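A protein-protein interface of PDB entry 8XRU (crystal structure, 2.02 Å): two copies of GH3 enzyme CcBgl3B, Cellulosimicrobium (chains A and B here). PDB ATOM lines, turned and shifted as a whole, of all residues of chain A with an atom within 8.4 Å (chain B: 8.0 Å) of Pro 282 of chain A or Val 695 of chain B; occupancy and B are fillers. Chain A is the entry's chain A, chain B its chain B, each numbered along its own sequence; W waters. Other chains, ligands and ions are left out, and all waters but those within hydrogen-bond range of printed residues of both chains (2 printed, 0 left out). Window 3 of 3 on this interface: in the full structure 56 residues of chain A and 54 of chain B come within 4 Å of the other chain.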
ATOM      1  N   MET A 274      19.543 -25.502  13.380  1.00  0.00           N
ATOM      2  CA  MET A 274      19.318 -25.763  11.958  1.00  0.00           C
ATOM      3  C   MET A 274      18.248 -26.827  11.751  1.00  0.00           C
ATOM      4  O   MET A 274      17.575 -26.835  10.714  1.00  0.00           O
ATOM      5  CB  MET A 274      20.628 -26.161  11.276  1.00  0.00           C
ATOM      6  CG  MET A 274      21.656 -25.030  11.274  1.00  0.00           C
ATOM      7  SD  MET A 274      23.072 -25.272  10.185  1.00  0.00           S
ATOM      8  CE  MET A 274      23.740 -26.797  10.852  1.00  0.00           C
ATOM      9  N   VAL A 275      18.054 -27.710  12.731  1.00  0.00           N
ATOM     10  CA  VAL A 275      16.974 -28.689  12.680  1.00  0.00           C
ATOM     11  C   VAL A 275      15.673 -28.089  13.212  1.00  0.00           C
ATOM     12  O   VAL A 275      14.689 -27.973  12.476  1.00  0.00           O
ATOM     13  CB  VAL A 275      17.332 -29.967  13.467  1.00  0.00           C
ATOM     14  CG1 VAL A 275      16.143 -30.925  13.485  1.00  0.00           C
ATOM     15  CG2 VAL A 275      18.568 -30.645  12.879  1.00  0.00           C
ATOM     16  N   TRP A 276      15.645 -27.710  14.496  1.00  0.00           N
ATOM     17  CA  TRP A 276      14.364 -27.471  15.158  1.00  0.00           C
ATOM     18  C   TRP A 276      13.876 -26.026  15.075  1.00  0.00           C
ATOM     19  O   TRP A 276      12.689 -25.774  15.324  1.00  0.00           O
ATOM     20  CB  TRP A 276      14.441 -27.915  16.638  1.00  0.00           C
ATOM     21  CG  TRP A 276      15.427 -27.141  17.503  1.00  0.00           C
ATOM     22  CD1 TRP A 276      16.727 -27.478  17.768  1.00  0.00           C
ATOM     23  CD2 TRP A 276      15.179 -25.916  18.226  1.00  0.00           C
ATOM     24  NE1 TRP A 276      17.309 -26.528  18.586  1.00  0.00           N
ATOM     25  CE2 TRP A 276      16.380 -25.565  18.884  1.00  0.00           C
ATOM     26  CE3 TRP A 276      14.065 -25.082  18.372  1.00  0.00           C
ATOM     27  CZ2 TRP A 276      16.492 -24.419  19.689  1.00  0.00           C
ATOM     28  CZ3 TRP A 276      14.178 -23.941  19.178  1.00  0.00           C
ATOM     29  CH2 TRP A 276      15.386 -23.621  19.814  1.00  0.00           C
ATOM     30  N   GLN A 278      15.401 -23.253  12.610  1.00  0.00           N
ATOM     31  CA  GLN A 278      15.475 -22.723  11.256  1.00  0.00           C
ATOM     32  C   GLN A 278      14.840 -23.651  10.228  1.00  0.00           C
ATOM     33  O   GLN A 278      14.437 -23.183   9.152  1.00  0.00           O
ATOM     34  CB  GLN A 278      16.941 -22.419  10.908  1.00  0.00           C
ATOM     35  CG  GLN A 278      17.418 -21.109  11.577  1.00  0.00           C
ATOM     36  CD  GLN A 278      18.915 -21.042  11.806  1.00  0.00           C
ATOM     37  OE1 GLN A 278      19.603 -22.064  11.803  1.00  0.00           O
ATOM     38  NE2 GLN A 278      19.430 -19.826  12.015  1.00  0.00           N
ATOM     39  N   HIS A 279      14.701 -24.942  10.557  1.00  0.00           N
ATOM     40  CA  HIS A 279      14.033 -25.930   9.707  1.00  0.00           C
ATOM     41  C   HIS A 279      14.716 -26.062   8.352  1.00  0.00           C
ATOM     42  O   HIS A 279      14.061 -26.136   7.318  1.00  0.00           O
ATOM     43  CB  HIS A 279      12.542 -25.615   9.544  1.00  0.00           C
ATOM     44  CG  HIS A 279      11.767 -25.750  10.818  1.00  0.00           C
ATOM     45  ND1 HIS A 279      11.553 -24.691  11.679  1.00  0.00           N
ATOM     46  CD2 HIS A 279      11.211 -26.831  11.410  1.00  0.00           C
ATOM     47  CE1 HIS A 279      10.869 -25.111  12.728  1.00  0.00           C
ATOM     48  NE2 HIS A 279      10.647 -26.405  12.588  1.00  0.00           N
ATOM     49  N   ILE A 280      16.047 -26.095   8.348  1.00  0.00           N
ATOM     50  CA  ILE A 280      16.789 -26.322   7.114  1.00  0.00           C
ATOM     51  C   ILE A 280      17.476 -27.676   7.071  1.00  0.00           C
ATOM     52  O   ILE A 280      17.977 -28.062   6.002  1.00  0.00           O
ATOM     53  CB  ILE A 280      17.818 -25.204   6.833  1.00  0.00           C
ATOM     54  CG1 ILE A 280      18.916 -25.181   7.895  1.00  0.00           C
ATOM     55  CG2 ILE A 280      17.142 -23.844   6.684  1.00  0.00           C
ATOM     56  CD1 ILE A 280      20.182 -24.528   7.376  1.00  0.00           C
ATOM     57  N   GLN A 281      17.526 -28.406   8.180  1.00  0.00           N
ATOM     58  CA  GLN A 281      18.051 -29.752   8.125  1.00  0.00           C
ATOM     59  C   GLN A 281      16.988 -30.738   8.594  1.00  0.00           C
ATOM     60  O   GLN A 281      16.243 -30.433   9.534  1.00  0.00           O
ATOM     61  CB  GLN A 281      19.310 -29.889   8.990  1.00  0.00           C
ATOM     62  CG  GLN A 281      20.534 -29.163   8.425  1.00  0.00           C
ATOM     63  CD  GLN A 281      21.083 -29.844   7.174  1.00  0.00           C
ATOM     64  OE1 GLN A 281      20.737 -30.984   6.887  1.00  0.00           O
ATOM     65  NE2 GLN A 281      21.942 -29.145   6.431  1.00  0.00           N
ATOM     66  N   PRO A 282      16.873 -31.907   7.949  1.00  0.00           N
ATOM     67  CA  PRO A 282      15.818 -32.854   8.351  1.00  0.00           C
ATOM     68  C   PRO A 282      16.073 -33.523   9.685  1.00  0.00           C
ATOM     69  O   PRO A 282      15.112 -33.954  10.333  1.00  0.00           O
ATOM     70  CB  PRO A 282      15.803 -33.884   7.204  1.00  0.00           C
ATOM     71  CG  PRO A 282      17.186 -33.837   6.626  1.00  0.00           C
ATOM     72  CD  PRO A 282      17.614 -32.374   6.758  1.00  0.00           C
ATOM     73  N   ASP A 283      17.330 -33.645  10.104  1.00  0.00           N
ATOM     74  CA  ASP A 283      17.672 -34.374  11.315  1.00  0.00           C
ATOM     75  C   ASP A 283      19.084 -34.003  11.739  1.00  0.00           C
ATOM     76  O   ASP A 283      19.810 -33.296  11.032  1.00  0.00           O
ATOM     77  CB  ASP A 283      17.540 -35.897  11.122  1.00  0.00           C
ATOM     78  CG  ASP A 283      18.289 -36.401   9.902  1.00  0.00           C
ATOM     79  OD1 ASP A 283      19.450 -35.995   9.676  1.00  0.00           O
ATOM     80  OD2 ASP A 283      17.728 -37.256   9.188  1.00  0.00           O
ATOM     81  N   TYR A 284      19.464 -34.510  12.910  1.00  0.00           N
ATOM     82  CA  TYR A 284      20.702 -34.094  13.554  1.00  0.00           C
ATOM     83  C   TYR A 284      21.936 -34.677  12.886  1.00  0.00           C
ATOM     84  O   TYR A 284      23.009 -34.070  12.950  1.00  0.00           O
ATOM     85  CB  TYR A 284      20.676 -34.487  15.038  1.00  0.00           C
ATOM     86  CG  TYR A 284      20.018 -33.442  15.897  1.00  0.00           C
ATOM     87  CD1 TYR A 284      18.629 -33.350  15.985  1.00  0.00           C
ATOM     88  CD2 TYR A 284      20.780 -32.512  16.582  1.00  0.00           C
ATOM     89  CE1 TYR A 284      18.028 -32.363  16.758  1.00  0.00           C
ATOM     90  CE2 TYR A 284      20.192 -31.548  17.358  1.00  0.00           C
ATOM     91  CZ  TYR A 284      18.821 -31.469  17.437  1.00  0.00           C
ATOM     92  OH  TYR A 284      18.263 -30.484  18.225  1.00  0.00           O
ATOM     93  N   VAL A 285      21.831 -35.863  12.282  1.00  0.00           N
ATOM     94  CA  VAL A 285      22.983 -36.397  11.561  1.00  0.00           C
ATOM     95  C   VAL A 285      23.291 -35.543  10.338  1.00  0.00           C
ATOM     96  O   VAL A 285      24.460 -35.286  10.025  1.00  0.00           O
ATOM     97  CB  VAL A 285      22.771 -37.888  11.202  1.00  0.00           C
ATOM     98  CG1 VAL A 285      21.606 -38.072  10.259  1.00  0.00           C
ATOM     99  CG2 VAL A 285      24.022 -38.448  10.518  1.00  0.00           C
ATOM    100  N   HIS A 286      22.258 -35.055   9.643  1.00  0.00           N
ATOM    101  CA  HIS A 286      22.523 -34.206   8.480  1.00  0.00           C
ATOM    102  C   HIS A 286      22.970 -32.802   8.895  1.00  0.00           C
ATOM    103  O   HIS A 286      23.779 -32.180   8.194  1.00  0.00           O
ATOM    104  CB  HIS A 286      21.288 -34.151   7.573  1.00  0.00           C
ATOM    105  CG  HIS A 286      21.135 -35.360   6.694  1.00  0.00           C
ATOM    106  ND1 HIS A 286      20.535 -36.522   7.129  1.00  0.00           N
ATOM    107  CD2 HIS A 286      21.524 -35.594   5.416  1.00  0.00           C
ATOM    108  CE1 HIS A 286      20.555 -37.418   6.156  1.00  0.00           C
ATOM    109  NE2 HIS A 286      21.149 -36.881   5.105  1.00  0.00           N
ATOM    110  N   ALA A 287      22.480 -32.293  10.033  1.00  0.00           N
ATOM    111  CA  ALA A 287      22.994 -31.022  10.552  1.00  0.00           C
ATOM    112  C   ALA A 287      24.450 -31.153  10.990  1.00  0.00           C
ATOM    113  O   ALA A 287      25.274 -30.277  10.704  1.00  0.00           O
ATOM    114  CB  ALA A 287      22.130 -30.539  11.718  1.00  0.00           C
ATOM    115  N   ALA A 290      26.662 -31.363   7.943  1.00  0.00           N
ATOM    116  CA  ALA A 290      26.784 -30.063   7.281  1.00  0.00           C
ATOM    117  C   ALA A 290      27.700 -29.119   8.056  1.00  0.00           C
ATOM    118  O   ALA A 290      28.474 -28.356   7.456  1.00  0.00           O
ATOM    119  CB  ALA A 290      25.400 -29.437   7.093  1.00  0.00           C
ATOM    120  N   ARG A 304      23.752 -33.559  20.789  1.00  0.00           N
ATOM    121  CA  ARG A 304      23.465 -34.576  19.787  1.00  0.00           C
ATOM    122  C   ARG A 304      24.416 -34.530  18.600  1.00  0.00           C
ATOM    123  O   ARG A 304      24.348 -35.419  17.741  1.00  0.00           O
ATOM    124  CB  ARG A 304      22.011 -34.452  19.326  1.00  0.00           C
ATOM    125  CG  ARG A 304      21.035 -34.719  20.478  1.00  0.00           C
ATOM    126  CD  ARG A 304      19.592 -34.667  20.037  1.00  0.00           C
ATOM    127  NE  ARG A 304      19.349 -35.547  18.899  1.00  0.00           N
ATOM    128  CZ  ARG A 304      18.144 -35.796  18.404  1.00  0.00           C
ATOM    129  NH1 ARG A 304      17.081 -35.231  18.963  1.00  0.00           N
ATOM    130  NH2 ARG A 304      18.002 -36.603  17.355  1.00  0.00           N
ATOM    131  N   ARG B 624      11.169 -18.027   8.922  1.00  0.00           N
ATOM    132  CA  ARG B 624      11.402 -18.724  10.179  1.00  0.00           C
ATOM    133  C   ARG B 624      12.806 -18.469  10.712  1.00  0.00           C
ATOM    134  O   ARG B 624      13.733 -18.145   9.965  1.00  0.00           O
ATOM    135  CB  ARG B 624      11.259 -20.242  10.005  1.00  0.00           C
ATOM    136  CG  ARG B 624       9.937 -20.751   9.538  1.00  0.00           C
ATOM    137  CD  ARG B 624      10.189 -22.128   8.903  1.00  0.00           C
ATOM    138  NE  ARG B 624       8.984 -22.896   8.619  1.00  0.00           N
ATOM    139  CZ  ARG B 624       8.839 -23.666   7.539  1.00  0.00           C
ATOM    140  NH1 ARG B 624       9.814 -23.740   6.647  1.00  0.00           N
ATOM    141  NH2 ARG B 624       7.719 -24.344   7.340  1.00  0.00           N
ATOM    142  N   SER B 692       2.829 -24.782   3.281  1.00  0.00           N
ATOM    143  CA  SER B 692       4.010 -24.693   4.123  1.00  0.00           C
ATOM    144  C   SER B 692       4.991 -25.781   3.720  1.00  0.00           C
ATOM    145  O   SER B 692       4.614 -26.953   3.614  1.00  0.00           O
ATOM    146  CB  SER B 692       3.640 -24.817   5.608  1.00  0.00           C
ATOM    147  OG  SER B 692       4.800 -24.752   6.412  1.00  0.00           O
ATOM    148  N   ASP B 693       6.245 -25.389   3.507  1.00  0.00           N
ATOM    149  CA  ASP B 693       7.337 -26.292   3.149  1.00  0.00           C
ATOM    150  C   ASP B 693       8.076 -26.636   4.440  1.00  0.00           C
ATOM    151  O   ASP B 693       8.721 -25.771   5.036  1.00  0.00           O
ATOM    152  CB  ASP B 693       8.254 -25.624   2.119  1.00  0.00           C
ATOM    153  CG  ASP B 693       9.253 -26.586   1.492  1.00  0.00           C
ATOM    154  OD1 ASP B 693       9.436 -27.674   2.061  1.00  0.00           O
ATOM    155  OD2 ASP B 693       9.865 -26.247   0.443  1.00  0.00           O
ATOM    156  N   THR B 694       7.990 -27.907   4.865  1.00  0.00           N
ATOM    157  CA  THR B 694       8.324 -28.265   6.243  1.00  0.00           C
ATOM    158  C   THR B 694       9.814 -28.131   6.534  1.00  0.00           C
ATOM    159  O   THR B 694      10.195 -27.648   7.608  1.00  0.00           O
ATOM    160  CB  THR B 694       7.840 -29.693   6.536  1.00  0.00           C
ATOM    161  OG1 THR B 694       6.449 -29.773   6.218  1.00  0.00           O
ATOM    162  CG2 THR B 694       8.028 -30.034   8.027  1.00  0.00           C
ATOM    163  N   VAL B 695      10.666 -28.545   5.598  1.00  0.00           N
ATOM    164  CA  VAL B 695      12.122 -28.505   5.734  1.00  0.00           C
ATOM    165  C   VAL B 695      12.667 -27.893   4.453  1.00  0.00           C
ATOM    166  O   VAL B 695      12.408 -28.416   3.368  1.00  0.00           O
ATOM    167  CB  VAL B 695      12.728 -29.909   5.949  1.00  0.00           C
ATOM    168  CG1 VAL B 695      14.250 -29.826   6.044  1.00  0.00           C
ATOM    169  CG2 VAL B 695      12.137 -30.607   7.188  1.00  0.00           C
ATOM    170  N   THR B 696      13.420 -26.798   4.556  1.00  0.00           N
ATOM    171  CA  THR B 696      13.837 -26.068   3.358  1.00  0.00           C
ATOM    172  C   THR B 696      15.357 -25.989   3.295  1.00  0.00           C
ATOM    173  O   THR B 696      16.021 -25.942   4.322  1.00  0.00           O
ATOM    174  CB  THR B 696      13.220 -24.674   3.352  1.00  0.00           C
ATOM    175  OG1 THR B 696      13.543 -23.991   4.580  1.00  0.00           O
ATOM    176  CG2 THR B 696      11.712 -24.786   3.237  1.00  0.00           C
ATOM    177  N   SER B 697      15.933 -26.005   2.091  1.00  0.00           N
ATOM    178  CA  SER B 697      17.396 -25.988   2.041  1.00  0.00           C
ATOM    179  C   SER B 697      17.961 -24.658   2.548  1.00  0.00           C
ATOM    180  O   SER B 697      19.103 -24.604   3.023  1.00  0.00           O
ATOM    181  CB  SER B 697      17.889 -26.272   0.624  1.00  0.00           C
ATOM    182  OG  SER B 697      17.612 -25.177  -0.227  1.00  0.00           O
ATOM    183  N   VAL B 698      17.182 -23.583   2.437  1.00  0.00           N
ATOM    184  CA  VAL B 698      17.499 -22.266   2.976  1.00  0.00           C
ATOM    185  C   VAL B 698      16.279 -21.819   3.772  1.00  0.00           C
ATOM    186  O   VAL B 698      15.168 -22.302   3.545  1.00  0.00           O
ATOM    187  CB  VAL B 698      17.832 -21.258   1.854  1.00  0.00           C
ATOM    188  CG1 VAL B 698      19.229 -21.517   1.288  1.00  0.00           C
ATOM    189  CG2 VAL B 698      16.835 -21.410   0.733  1.00  0.00           C
ATOM    190  N   THR B 699      16.480 -20.898   4.725  1.00  0.00           N
ATOM    191  CA  THR B 699      15.331 -20.470   5.521  1.00  0.00           C
ATOM    192  C   THR B 699      14.266 -19.857   4.622  1.00  0.00           C
ATOM    193  O   THR B 699      14.564 -19.241   3.589  1.00  0.00           O
ATOM    194  CB  THR B 699      15.720 -19.467   6.622  1.00  0.00           C
ATOM    195  OG1 THR B 699      16.400 -18.329   6.066  1.00  0.00           O
ATOM    196  CG2 THR B 699      16.594 -20.130   7.649  1.00  0.00           C
ATOM    197  N   TRP B 700      13.008 -20.039   5.014  1.00  0.00           N
ATOM    198  CA  TRP B 700      11.909 -19.679   4.128  1.00  0.00           C
ATOM    199  C   TRP B 700      10.724 -19.244   4.978  1.00  0.00           C
ATOM    200  O   TRP B 700      10.741 -19.357   6.206  1.00  0.00           O
ATOM    201  CB  TRP B 700      11.553 -20.861   3.188  1.00  0.00           C
ATOM    202  CG  TRP B 700      10.705 -20.450   1.997  1.00  0.00           C
ATOM    203  CD1 TRP B 700       9.420 -20.835   1.738  1.00  0.00           C
ATOM    204  CD2 TRP B 700      11.073 -19.547   0.936  1.00  0.00           C
ATOM    205  NE1 TRP B 700       8.971 -20.242   0.578  1.00  0.00           N
ATOM    206  CE2 TRP B 700       9.966 -19.452   0.063  1.00  0.00           C
ATOM    207  CE3 TRP B 700      12.232 -18.822   0.633  1.00  0.00           C
ATOM    208  CZ2 TRP B 700       9.980 -18.649  -1.089  1.00  0.00           C
ATOM    209  CZ3 TRP B 700      12.243 -18.025  -0.516  1.00  0.00           C
ATOM    210  CH2 TRP B 700      11.122 -17.946  -1.360  1.00  0.00           C
ATOM    211  N   LEU B 732      10.475 -22.579  -3.641  1.00  0.00           N
ATOM    212  CA  LEU B 732      11.247 -21.592  -2.905  1.00  0.00           C
ATOM    213  C   LEU B 732      12.397 -21.135  -3.794  1.00  0.00           C
ATOM    214  O   LEU B 732      12.666 -21.727  -4.842  1.00  0.00           O
ATOM    215  CB  LEU B 732      11.768 -22.152  -1.561  1.00  0.00           C
ATOM    216  CG  LEU B 732      12.620 -23.421  -1.530  1.00  0.00           C
ATOM    217  CD1 LEU B 732      14.046 -23.176  -2.019  1.00  0.00           C
ATOM    218  CD2 LEU B 732      12.668 -23.944  -0.089  1.00  0.00           C
ATOM    219  N   GLU B 742      11.492 -28.297  -4.035  1.00  0.00           N
ATOM    220  CA  GLU B 742      12.379 -29.271  -3.431  1.00  0.00           C
ATOM    221  C   GLU B 742      11.562 -30.466  -2.959  1.00  0.00           C
ATOM    222  O   GLU B 742      10.513 -30.280  -2.330  1.00  0.00           O
ATOM    223  CB  GLU B 742      13.139 -28.662  -2.255  1.00  0.00           C
ATOM    224  CG  GLU B 742      13.942 -27.406  -2.629  1.00  0.00           C
ATOM    225  CD  GLU B 742      14.850 -26.918  -1.506  1.00  0.00           C
ATOM    226  OE1 GLU B 742      14.509 -27.117  -0.318  1.00  0.00           O
ATOM    227  OE2 GLU B 742      15.919 -26.350  -1.819  1.00  0.00           O
ATOM    228  N   PRO B 743      11.993 -31.692  -3.249  1.00  0.00           N
ATOM    229  CA  PRO B 743      11.280 -32.864  -2.715  1.00  0.00           C
ATOM    230  C   PRO B 743      11.252 -32.847  -1.193  1.00  0.00           C
ATOM    231  O   PRO B 743      12.191 -32.387  -0.537  1.00  0.00           O
ATOM    232  CB  PRO B 743      12.092 -34.053  -3.242  1.00  0.00           C
ATOM    233  CG  PRO B 743      12.905 -33.513  -4.375  1.00  0.00           C
ATOM    234  CD  PRO B 743      13.175 -32.063  -4.043  1.00  0.00           C
ATOM    235  N   GLY B 744      10.161 -33.361  -0.633  1.00  0.00           N
ATOM    236  CA  GLY B 744      10.027 -33.501   0.801  1.00  0.00           C
ATOM    237  C   GLY B 744       8.581 -33.314   1.213  1.00  0.00           C
ATOM    238  O   GLY B 744       7.676 -33.412   0.387  1.00  0.00           O
ATOM    239  N   GLU B 745       8.404 -33.009   2.500  1.00  0.00           N
ATOM    240  CA  GLU B 745       7.089 -32.861   3.106  1.00  0.00           C
ATOM    241  C   GLU B 745       6.587 -31.429   2.989  1.00  0.00           C
ATOM    242  O   GLU B 745       7.358 -30.468   3.029  1.00  0.00           O
ATOM    243  CB  GLU B 745       7.114 -33.240   4.598  1.00  0.00           C
ATOM    244  CG  GLU B 745       7.578 -34.639   4.923  1.00  0.00           C
ATOM    245  CD  GLU B 745       7.218 -35.032   6.356  1.00  0.00           C
ATOM    246  OE1 GLU B 745       7.114 -34.120   7.221  1.00  0.00           O
ATOM    247  OE2 GLU B 745       7.039 -36.245   6.615  1.00  0.00           O
ATOM    248  N   PHE B 746       5.266 -31.304   2.916  1.00  0.00           N
ATOM    249  CA  PHE B 746       4.581 -30.025   2.883  1.00  0.00           C
ATOM    250  C   PHE B 746       3.324 -30.144   3.731  1.00  0.00           C
ATOM    251  O   PHE B 746       2.862 -31.250   4.025  1.00  0.00           O
ATOM    252  CB  PHE B 746       4.170 -29.623   1.457  1.00  0.00           C
ATOM    253  CG  PHE B 746       5.315 -29.365   0.510  1.00  0.00           C
ATOM    254  CD1 PHE B 746       5.964 -30.417  -0.129  1.00  0.00           C
ATOM    255  CD2 PHE B 746       5.684 -28.059   0.189  1.00  0.00           C
ATOM    256  CE1 PHE B 746       6.990 -30.178  -1.043  1.00  0.00           C
ATOM    257  CE2 PHE B 746       6.707 -27.799  -0.725  1.00  0.00           C
ATOM    258  CZ  PHE B 746       7.366 -28.855  -1.341  1.00  0.00           C
HETATM  259  O   HOH W   1      12.882 -22.620   6.906  1.00  0.00           O
HETATM  260  O   HOH W   2      20.362 -26.778   4.055  1.00  0.00           O
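No position is printed for both chains.
O of Met 274 of chain A lies within hydrogen-bond range of N of His 279 of chain A, 3.4 Å away. The backbone NH (N) of Ile 280 of chain A lies within hydrogen-bond range of the backbone carbonyl oxygen (O) of Met 274 of chain A, at 2.9 Å. The backbone carbonyl oxygen (O) of Met 274 of chain A is in hydrogen-bond range of the backbone NH (N) of Gln 281 of chain A (3.0 Å). O of Trp 276 of chain A lies close to NE2 of His 279 of chain A. The backbone NH of Thr 694 of chain B sits at hydrogen-bond distance from the backbone carbonyl oxygen of Glu 745 of chain B (3.2 Å). OG1 of Thr 696 of chain B lies within hydrogen-bond range of O of Val 698 of chain B.
Among the printed residues, pairs that only touch across the chains: Gln 278 of chain A with Thr 699 of chain B, His 279 of chain A with Thr 694 of chain B, His 279 of chain A with Val 695 of chain B, Ile 280 of chain A with Val 698 of chain B, Ile 280 of chain A with Thr 699 of chain B, Gln 281 of chain A with Val 695 of chain B and Pro 282 of chain A with Val 695 of chain B.
Water W2 lies within hydrogen-bond range of the backbone carbonyl oxygen (O) of Ser 697 of chain B (2.7 Å) and the backbone carbonyl oxygen (O) of Ile 280 of chain A (3.3 Å). Water W1 lies within hydrogen-bond range of the side-chain hydroxyl (OG1) of Thr 696 of chain B, the backbone carbonyl oxygen (O) of Gln 278 of chain A, the backbone NH (N) of Trp 700 of chain B and the guanidinium group (NH1) of Arg 624 of chain B.
Of the 16 printed residues of chain B, 5 touch a printed residue of chain A. Hydrophobic or aromatic side chains of chain A within 4 Å of the printed part of chain B: His 279 and Ile 280. Among the printed residues, 9 pairs touch across the chains. Among the printed residues, no Asp or Glu carboxylate lies within 4 Å of a Lys or Arg side-chain nitrogen of the other chain.
The backbone carbonyl oxygen (O) of His 279 of chain A sits at hydrogen-bond distance from the backbone NH (N) of Thr 696 of chain B, at 2.9 Å. O of Ile 280 of chain A sits close to O of Thr 696 of chain B.
Of chain B, only Val 695 comes within 4 Å of Pro 282 of chain A. Of the printed residues of chain A, Val 695 of chain B touches His 279 (3.4 Å), Gln 281 (3.9 Å) and Pro 282 (3.9 Å). Thr 696 of chain B touches just these residues of chain A: His 279 (2.9 Å) and Ile 280 (2.9 Å). Of the printed residues of chain B, Gln 278 of chain A touches Thr 699. Of the printed residues of chain B, Gln 281 of chain A touches Val 695 (3.9 Å). Printed residues of chain A within 4 Å of Val 698 of chain B: Ile 280 (3.7 Å). Ser 697 of chain B touches none of the printed residues of chain A. Val 275 of chain A touches none of the printed residues of chain B. The nearest residue of chain B that does not touch Pro 282 of chain A is Thr 696 of chain B (7.0 Å). The nearest printed residue of chain A that does not touch Val 695 of chain B is Ile 280 of chain A (4.01 Å). The nearest printed residue of chain B that does not touch Gln 281 of chain A is Thr 696 of chain B (4.8 Å).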
